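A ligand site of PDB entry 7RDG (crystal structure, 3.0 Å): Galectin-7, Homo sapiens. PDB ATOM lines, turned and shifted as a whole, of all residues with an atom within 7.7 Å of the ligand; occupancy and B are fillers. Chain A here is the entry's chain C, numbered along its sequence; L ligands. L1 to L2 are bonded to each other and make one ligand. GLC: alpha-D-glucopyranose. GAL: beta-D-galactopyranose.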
ATOM      1  N   ARG A  31     -14.079  -9.264 -25.555  1.00  0.00           N
ATOM      2  CA  ARG A  31     -13.667 -10.504 -24.906  1.00  0.00           C
ATOM      3  C   ARG A  31     -14.764 -11.007 -23.985  1.00  0.00           C
ATOM      4  O   ARG A  31     -15.622 -10.247 -23.520  1.00  0.00           O
ATOM      5  CB  ARG A  31     -12.361 -10.287 -24.110  1.00  0.00           C
ATOM      6  CG  ARG A  31     -12.354  -9.033 -23.304  1.00  0.00           C
ATOM      7  CD  ARG A  31     -11.049  -8.854 -22.577  1.00  0.00           C
ATOM      8  NE  ARG A  31      -9.984  -8.475 -23.505  1.00  0.00           N
ATOM      9  CZ  ARG A  31      -8.701  -8.344 -23.187  1.00  0.00           C
ATOM     10  NH1 ARG A  31      -8.286  -8.530 -21.924  1.00  0.00           N
ATOM     11  NH2 ARG A  31      -7.831  -8.041 -24.130  1.00  0.00           N
ATOM     12  N   PHE A  32     -14.745 -12.316 -23.698  1.00  0.00           N
ATOM     13  CA  PHE A  32     -15.614 -12.847 -22.661  1.00  0.00           C
ATOM     14  C   PHE A  32     -14.866 -13.865 -21.840  1.00  0.00           C
ATOM     15  O   PHE A  32     -13.691 -14.162 -22.094  1.00  0.00           O
ATOM     16  CB  PHE A  32     -16.912 -13.449 -23.195  1.00  0.00           C
ATOM     17  CG  PHE A  32     -16.764 -14.700 -24.023  1.00  0.00           C
ATOM     18  CD1 PHE A  32     -16.581 -14.612 -25.392  1.00  0.00           C
ATOM     19  CD2 PHE A  32     -16.896 -15.949 -23.450  1.00  0.00           C
ATOM     20  CE1 PHE A  32     -16.518 -15.776 -26.171  1.00  0.00           C
ATOM     21  CE2 PHE A  32     -16.832 -17.086 -24.210  1.00  0.00           C
ATOM     22  CZ  PHE A  32     -16.640 -17.009 -25.565  1.00  0.00           C
ATOM     23  N   HIS A  33     -15.525 -14.364 -20.801  1.00  0.00           N
ATOM     24  CA  HIS A  33     -14.792 -15.241 -19.900  1.00  0.00           C
ATOM     25  C   HIS A  33     -15.651 -16.339 -19.318  1.00  0.00           C
ATOM     26  O   HIS A  33     -16.871 -16.210 -19.192  1.00  0.00           O
ATOM     27  CB  HIS A  33     -14.132 -14.439 -18.769  1.00  0.00           C
ATOM     28  CG  HIS A  33     -15.091 -13.586 -18.001  1.00  0.00           C
ATOM     29  ND1 HIS A  33     -15.190 -12.222 -18.195  1.00  0.00           N
ATOM     30  CD2 HIS A  33     -15.995 -13.915 -17.053  1.00  0.00           C
ATOM     31  CE1 HIS A  33     -16.127 -11.752 -17.385  1.00  0.00           C
ATOM     32  NE2 HIS A  33     -16.626 -12.753 -16.678  1.00  0.00           N
ATOM     33  N   HIS A  49      -9.606 -19.811 -15.323  1.00  0.00           N
ATOM     34  CA  HIS A  49     -10.013 -18.588 -16.015  1.00  0.00           C
ATOM     35  C   HIS A  49      -9.821 -18.842 -17.501  1.00  0.00           C
ATOM     36  O   HIS A  49      -8.696 -18.995 -17.985  1.00  0.00           O
ATOM     37  CB  HIS A  49      -9.205 -17.401 -15.463  1.00  0.00           C
ATOM     38  CG  HIS A  49      -9.407 -16.113 -16.198  1.00  0.00           C
ATOM     39  ND1 HIS A  49     -10.547 -15.357 -16.044  1.00  0.00           N
ATOM     40  CD2 HIS A  49      -8.561 -15.389 -16.960  1.00  0.00           C
ATOM     41  CE1 HIS A  49     -10.434 -14.254 -16.761  1.00  0.00           C
ATOM     42  NE2 HIS A  49      -9.230 -14.246 -17.329  1.00  0.00           N
ATOM     43  N   PHE A  50     -10.938 -18.980 -18.206  1.00  0.00           N
ATOM     44  CA  PHE A  50     -11.004 -19.329 -19.620  1.00  0.00           C
ATOM     45  C   PHE A  50     -11.431 -18.023 -20.326  1.00  0.00           C
ATOM     46  O   PHE A  50     -12.569 -17.599 -20.178  1.00  0.00           O
ATOM     47  CB  PHE A  50     -11.990 -20.519 -19.854  1.00  0.00           C
ATOM     48  CG  PHE A  50     -12.220 -20.795 -21.328  1.00  0.00           C
ATOM     49  CD1 PHE A  50     -11.327 -21.549 -22.036  1.00  0.00           C
ATOM     50  CD2 PHE A  50     -13.277 -20.221 -22.002  1.00  0.00           C
ATOM     51  CE1 PHE A  50     -11.475 -21.721 -23.397  1.00  0.00           C
ATOM     52  CE2 PHE A  50     -13.419 -20.402 -23.373  1.00  0.00           C
ATOM     53  CZ  PHE A  50     -12.502 -21.148 -24.065  1.00  0.00           C
ATOM     54  N   ASN A  51     -10.540 -17.378 -21.075  1.00  0.00           N
ATOM     55  CA  ASN A  51     -10.747 -15.976 -21.475  1.00  0.00           C
ATOM     56  C   ASN A  51     -10.430 -15.663 -22.937  1.00  0.00           C
ATOM     57  O   ASN A  51      -9.364 -15.113 -23.229  1.00  0.00           O
ATOM     58  CB  ASN A  51      -9.925 -15.048 -20.566  1.00  0.00           C
ATOM     59  CG  ASN A  51     -10.123 -13.582 -20.885  1.00  0.00           C
ATOM     60  OD1 ASN A  51      -9.180 -12.787 -20.839  1.00  0.00           O
ATOM     61  ND2 ASN A  51     -11.357 -13.218 -21.217  1.00  0.00           N
ATOM     62  N   ARG A  53     -10.164 -13.587 -26.142  1.00  0.00           N
ATOM     63  CA  ARG A  53     -10.115 -12.154 -26.475  1.00  0.00           C
ATOM     64  C   ARG A  53     -10.213 -12.059 -27.980  1.00  0.00           C
ATOM     65  O   ARG A  53      -9.321 -12.560 -28.611  1.00  0.00           O
ATOM     66  CB  ARG A  53      -8.839 -11.553 -25.869  1.00  0.00           C
ATOM     67  CG  ARG A  53      -8.702 -11.780 -24.357  1.00  0.00           C
ATOM     68  CD  ARG A  53      -7.255 -11.512 -23.932  1.00  0.00           C
ATOM     69  NE  ARG A  53      -6.964 -11.849 -22.546  1.00  0.00           N
ATOM     70  CZ  ARG A  53      -5.794 -11.575 -21.925  1.00  0.00           C
ATOM     71  NH1 ARG A  53      -4.814 -10.932 -22.584  1.00  0.00           N
ATOM     72  NH2 ARG A  53      -5.633 -11.943 -20.652  1.00  0.00           N
ATOM     73  N   THR A  56      -7.834  -8.972 -29.326  1.00  0.00           N
ATOM     74  CA  THR A  56      -6.437  -9.250 -29.510  1.00  0.00           C
ATOM     75  C   THR A  56      -6.167 -10.649 -30.077  1.00  0.00           C
ATOM     76  O   THR A  56      -4.993 -11.011 -30.262  1.00  0.00           O
ATOM     77  CB  THR A  56      -5.708  -9.080 -28.177  1.00  0.00           C
ATOM     78  OG1 THR A  56      -6.174 -10.080 -27.269  1.00  0.00           O
ATOM     79  CG2 THR A  56      -5.982  -7.712 -27.615  1.00  0.00           C
ATOM     80  N   GLU A  58      -6.351 -13.854 -29.109  1.00  0.00           N
ATOM     81  CA  GLU A  58      -5.790 -14.926 -28.307  1.00  0.00           C
ATOM     82  C   GLU A  58      -6.934 -15.491 -27.467  1.00  0.00           C
ATOM     83  O   GLU A  58      -7.964 -14.835 -27.277  1.00  0.00           O
ATOM     84  CB  GLU A  58      -4.633 -14.441 -27.433  1.00  0.00           C
ATOM     85  CG  GLU A  58      -4.985 -13.256 -26.510  1.00  0.00           C
ATOM     86  CD  GLU A  58      -3.800 -12.249 -26.302  1.00  0.00           C
ATOM     87  OE1 GLU A  58      -2.715 -12.477 -26.893  1.00  0.00           O
ATOM     88  OE2 GLU A  58      -3.970 -11.264 -25.531  1.00  0.00           O
ATOM     89  N   VAL A  60      -6.832 -17.127 -23.582  1.00  0.00           N
ATOM     90  CA  VAL A  60      -5.916 -17.177 -22.462  1.00  0.00           C
ATOM     91  C   VAL A  60      -6.497 -18.097 -21.391  1.00  0.00           C
ATOM     92  O   VAL A  60      -7.666 -17.974 -21.037  1.00  0.00           O
ATOM     93  CB  VAL A  60      -5.634 -15.767 -21.880  1.00  0.00           C
ATOM     94  CG1 VAL A  60      -5.081 -15.884 -20.441  1.00  0.00           C
ATOM     95  CG2 VAL A  60      -4.658 -15.018 -22.771  1.00  0.00           C
ATOM     96  N   PHE A  61      -5.642 -18.954 -20.855  1.00  0.00           N
ATOM     97  CA  PHE A  61      -5.954 -19.790 -19.716  1.00  0.00           C
ATOM     98  C   PHE A  61      -5.035 -19.578 -18.514  1.00  0.00           C
ATOM     99  O   PHE A  61      -3.816 -19.555 -18.647  1.00  0.00           O
ATOM    100  CB  PHE A  61      -5.736 -21.283 -20.060  1.00  0.00           C
ATOM    101  CG  PHE A  61      -6.589 -21.800 -21.195  1.00  0.00           C
ATOM    102  CD1 PHE A  61      -6.388 -21.370 -22.496  1.00  0.00           C
ATOM    103  CD2 PHE A  61      -7.554 -22.751 -20.956  1.00  0.00           C
ATOM    104  CE1 PHE A  61      -7.157 -21.884 -23.548  1.00  0.00           C
ATOM    105  CE2 PHE A  61      -8.329 -23.278 -22.000  1.00  0.00           C
ATOM    106  CZ  PHE A  61      -8.135 -22.827 -23.294  1.00  0.00           C
ATOM    107  N   ASN A  62      -5.629 -19.440 -17.333  1.00  0.00           N
ATOM    108  CA  ASN A  62      -4.854 -19.260 -16.108  1.00  0.00           C
ATOM    109  C   ASN A  62      -5.765 -19.498 -14.897  1.00  0.00           C
ATOM    110  O   ASN A  62      -6.974 -19.742 -15.021  1.00  0.00           O
ATOM    111  CB  ASN A  62      -4.349 -17.833 -16.161  1.00  0.00           C
ATOM    112  CG  ASN A  62      -3.149 -17.626 -15.340  1.00  0.00           C
ATOM    113  OD1 ASN A  62      -2.777 -18.497 -14.534  1.00  0.00           O
ATOM    114  ND2 ASN A  62      -2.535 -16.460 -15.509  1.00  0.00           N
ATOM    115  N   SER A  63      -5.142 -19.448 -13.727  1.00  0.00           N
ATOM    116  CA  SER A  63      -5.730 -19.557 -12.411  1.00  0.00           C
ATOM    117  C   SER A  63      -5.237 -18.403 -11.523  1.00  0.00           C
ATOM    118  O   SER A  63      -4.216 -17.730 -11.797  1.00  0.00           O
ATOM    119  CB  SER A  63      -5.343 -20.885 -11.777  1.00  0.00           C
ATOM    120  OG  SER A  63      -3.937 -20.994 -11.781  1.00  0.00           O
ATOM    121  N   LYS A  64      -5.977 -18.175 -10.429  1.00  0.00           N
ATOM    122  CA  LYS A  64      -5.690 -17.096  -9.449  1.00  0.00           C
ATOM    123  C   LYS A  64      -5.613 -17.728  -8.062  1.00  0.00           C
ATOM    124  O   LYS A  64      -6.399 -18.600  -7.781  1.00  0.00           O
ATOM    125  CB  LYS A  64      -6.770 -16.000  -9.480  1.00  0.00           C
ATOM    126  CG  LYS A  64      -6.392 -14.655  -8.828  1.00  0.00           C
ATOM    127  CD  LYS A  64      -6.966 -13.395  -9.602  1.00  0.00           C
ATOM    128  CE  LYS A  64      -8.439 -13.094  -9.335  1.00  0.00           C
ATOM    129  NZ  LYS A  64      -9.108 -12.350 -10.471  1.00  0.00           N
ATOM    130  N   TRP A  69      -2.363 -13.745 -10.417  1.00  0.00           N
ATOM    131  CA  TRP A  69      -2.463 -14.703 -11.500  1.00  0.00           C
ATOM    132  C   TRP A  69      -1.272 -15.659 -11.506  1.00  0.00           C
ATOM    133  O   TRP A  69      -0.178 -15.356 -10.993  1.00  0.00           O
ATOM    134  CB  TRP A  69      -2.572 -13.989 -12.865  1.00  0.00           C
ATOM    135  CG  TRP A  69      -3.861 -13.244 -13.007  1.00  0.00           C
ATOM    136  CD1 TRP A  69      -4.032 -11.889 -12.974  1.00  0.00           C
ATOM    137  CD2 TRP A  69      -5.169 -13.813 -13.175  1.00  0.00           C
ATOM    138  NE1 TRP A  69      -5.358 -11.576 -13.123  1.00  0.00           N
ATOM    139  CE2 TRP A  69      -6.083 -12.732 -13.248  1.00  0.00           C
ATOM    140  CE3 TRP A  69      -5.662 -15.118 -13.299  1.00  0.00           C
ATOM    141  CZ2 TRP A  69      -7.466 -12.922 -13.411  1.00  0.00           C
ATOM    142  CZ3 TRP A  69      -7.037 -15.304 -13.451  1.00  0.00           C
ATOM    143  CH2 TRP A  69      -7.922 -14.221 -13.501  1.00  0.00           C
ATOM    144  N   GLY A  70      -1.521 -16.857 -12.048  1.00  0.00           N
ATOM    145  CA  GLY A  70      -0.492 -17.877 -12.196  1.00  0.00           C
ATOM    146  C   GLY A  70       0.214 -17.666 -13.522  1.00  0.00           C
ATOM    147  O   GLY A  70       0.095 -16.597 -14.116  1.00  0.00           O
ATOM    148  N   ARG A  71       0.892 -18.704 -14.025  1.00  0.00           N
ATOM    149  CA  ARG A  71       1.497 -18.596 -15.353  1.00  0.00           C
ATOM    150  C   ARG A  71       0.399 -18.683 -16.413  1.00  0.00           C
ATOM    151  O   ARG A  71      -0.429 -19.612 -16.380  1.00  0.00           O
ATOM    152  CB  ARG A  71       2.567 -19.687 -15.578  1.00  0.00           C
ATOM    153  CG  ARG A  71       3.894 -19.701 -14.746  1.00  0.00           C
ATOM    154  CD  ARG A  71       4.994 -20.809 -15.031  1.00  0.00           C
ATOM    155  NE  ARG A  71       6.187 -20.804 -14.164  1.00  0.00           N
ATOM    156  CZ  ARG A  71       7.163 -21.728 -14.180  1.00  0.00           C
ATOM    157  NH1 ARG A  71       7.098 -22.754 -15.039  1.00  0.00           N
ATOM    158  NH2 ARG A  71       8.214 -21.631 -13.359  1.00  0.00           N
ATOM    159  N   GLU A  72       0.362 -17.754 -17.371  1.00  0.00           N
ATOM    160  CA  GLU A  72      -0.664 -17.845 -18.400  1.00  0.00           C
ATOM    161  C   GLU A  72      -0.390 -18.960 -19.418  1.00  0.00           C
ATOM    162  O   GLU A  72       0.748 -19.193 -19.811  1.00  0.00           O
ATOM    163  CB  GLU A  72      -0.747 -16.527 -19.140  1.00  0.00           C
ATOM    164  CG  GLU A  72      -1.147 -15.365 -18.283  1.00  0.00           C
ATOM    165  CD  GLU A  72      -1.430 -14.133 -19.112  1.00  0.00           C
ATOM    166  OE1 GLU A  72      -0.553 -13.714 -19.910  1.00  0.00           O
ATOM    167  OE2 GLU A  72      -2.556 -13.623 -18.984  1.00  0.00           O
ATOM    168  N   GLU A  73      -1.468 -19.601 -19.881  1.00  0.00           N
ATOM    169  CA  GLU A  73      -1.433 -20.551 -20.982  1.00  0.00           C
ATOM    170  C   GLU A  73      -2.307 -20.023 -22.123  1.00  0.00           C
ATOM    171  O   GLU A  73      -3.354 -19.417 -21.886  1.00  0.00           O
ATOM    172  CB  GLU A  73      -1.906 -21.944 -20.522  1.00  0.00           C
ATOM    173  CG  GLU A  73      -1.014 -22.494 -19.422  1.00  0.00           C
ATOM    174  CD  GLU A  73      -1.219 -23.972 -19.152  1.00  0.00           C
ATOM    175  OE1 GLU A  73      -1.947 -24.644 -19.936  1.00  0.00           O
ATOM    176  OE2 GLU A  73      -0.578 -24.484 -18.201  1.00  0.00           O
ATOM    177  N   ARG A  74      -1.856 -20.211 -23.366  1.00  0.00           N
ATOM    178  CA  ARG A  74      -2.556 -19.693 -24.538  1.00  0.00           C
ATOM    179  C   ARG A  74      -2.875 -20.815 -25.527  1.00  0.00           C
ATOM    180  O   ARG A  74      -1.966 -21.502 -25.990  1.00  0.00           O
ATOM    181  CB  ARG A  74      -1.724 -18.599 -25.245  1.00  0.00           C
ATOM    182  CG  ARG A  74      -1.830 -17.238 -24.566  1.00  0.00           C
ATOM    183  CD  ARG A  74      -0.855 -16.265 -25.189  1.00  0.00           C
ATOM    184  NE  ARG A  74      -1.281 -14.892 -24.980  1.00  0.00           N
ATOM    185  CZ  ARG A  74      -1.246 -14.274 -23.807  1.00  0.00           C
ATOM    186  NH1 ARG A  74      -0.806 -14.917 -22.722  1.00  0.00           N
ATOM    187  NH2 ARG A  74      -1.655 -13.010 -23.727  1.00  0.00           N
HETATM  188  C1  GLC L   1       0.215  -9.485 -19.875  1.00  0.00           C
HETATM  189  C2  GLC L   1      -0.683 -10.630 -20.350  1.00  0.00           C
HETATM  190  C3  GLC L   1      -2.125 -10.300 -20.196  1.00  0.00           C
HETATM  191  C4  GLC L   1      -2.482  -9.938 -18.772  1.00  0.00           C
HETATM  192  C5  GLC L   1      -1.717  -8.633 -18.473  1.00  0.00           C
HETATM  193  C6  GLC L   1      -1.866  -8.028 -17.110  1.00  0.00           C
HETATM  194  O1  GLC L   1       0.265  -8.462 -20.800  1.00  0.00           O
HETATM  195  O2  GLC L   1      -0.255 -10.962 -21.690  1.00  0.00           O
HETATM  196  O3  GLC L   1      -2.863 -11.431 -20.772  1.00  0.00           O
HETATM  197  O4  GLC L   1      -3.866  -9.697 -18.846  1.00  0.00           O
HETATM  198  O5  GLC L   1      -0.254  -8.790 -18.620  1.00  0.00           O
HETATM  199  O6  GLC L   1      -1.645  -6.617 -17.270  1.00  0.00           O
HETATM  200  C1  GAL L   2      -4.574 -10.125 -17.724  1.00  0.00           C
HETATM  201  C2  GAL L   2      -5.997  -9.587 -17.790  1.00  0.00           C
HETATM  202  C3  GAL L   2      -6.886 -10.240 -16.796  1.00  0.00           C
HETATM  203  C4  GAL L   2      -6.925 -11.724 -17.121  1.00  0.00           C
HETATM  204  C5  GAL L   2      -5.574 -12.337 -16.861  1.00  0.00           C
HETATM  205  C6  GAL L   2      -5.336 -13.760 -17.351  1.00  0.00           C
HETATM  206  O2  GAL L   2      -5.758  -8.185 -17.562  1.00  0.00           O
HETATM  207  O3  GAL L   2      -8.252  -9.792 -16.781  1.00  0.00           O
HETATM  208  O4  GAL L   2      -7.298 -12.021 -18.468  1.00  0.00           O
HETATM  209  O5  GAL L   2      -4.481 -11.627 -17.552  1.00  0.00           O
HETATM  210  O6  GAL L   2      -4.013 -14.152 -17.101  1.00  0.00           O
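O6 of GAL L2 is in hydrogen-bond range of OE2 of Glu 72 (2.4 Å). The guanidinium group (NH1) of Arg 53 sits at hydrogen-bond distance from an oxygen (O3) of GLC L1 (2.7 Å). The side-chain amide oxygen (OD1) of Asn 51 sits at hydrogen-bond distance from an oxygen (O4) of GAL L2, 3.1 Å away. A ring nitrogen (NE2) of His 49 lies within hydrogen-bond range of an oxygen (O4) of GAL L2 (3.2 Å). ND2 of Asn 62 sits at hydrogen-bond distance from O6 of GAL L2 (3.2 Å). An oxygen (O2) of GLC L1 lies within hydrogen-bond range of the guanidinium group of Arg 74, 3.2 Å away.
Residues that only touch the ligand: Trp 69 and Val 60. Hydrophobic or aromatic side chains within 4 Å of the ligand: His 49, Val 60 and Trp 69. Eight residues have an atom within 4 Å of the ligand: His 49, Asn 51, Arg 53, Val 60, Asn 62, Trp 69, Glu 72 and Arg 74.
The side-chain carboxylate (OE2) of Glu 72 is in salt-bridge range of the guanidinium group (NH2) of Arg 53, at 3.9 Å. The side-chain carboxylate (OE1) of Glu 72 lies within salt-bridge range of the guanidinium group (NH1) of Arg 74. The guanidinium group (NE) of Arg 53 lies within hydrogen-bond range of the side-chain amide oxygen (OD1) of Asn 51 (3.0 Å). O of Val 60 is in hydrogen-bond range of N of Asn 51 (2.9 Å). ND2 of Asn 51 lies within hydrogen-bond range of O of Phe 32. The backbone NH (N) of His 49 is in hydrogen-bond range of the backbone carbonyl oxygen (O) of Asn 62 (2.7 Å). ND2 of Asn 62 is in hydrogen-bond range of O of Gly 70, at 3.0 Å. NH2 of Arg 74 lies within salt-bridge range of OE1 of Glu 58, at 3.4 Å.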
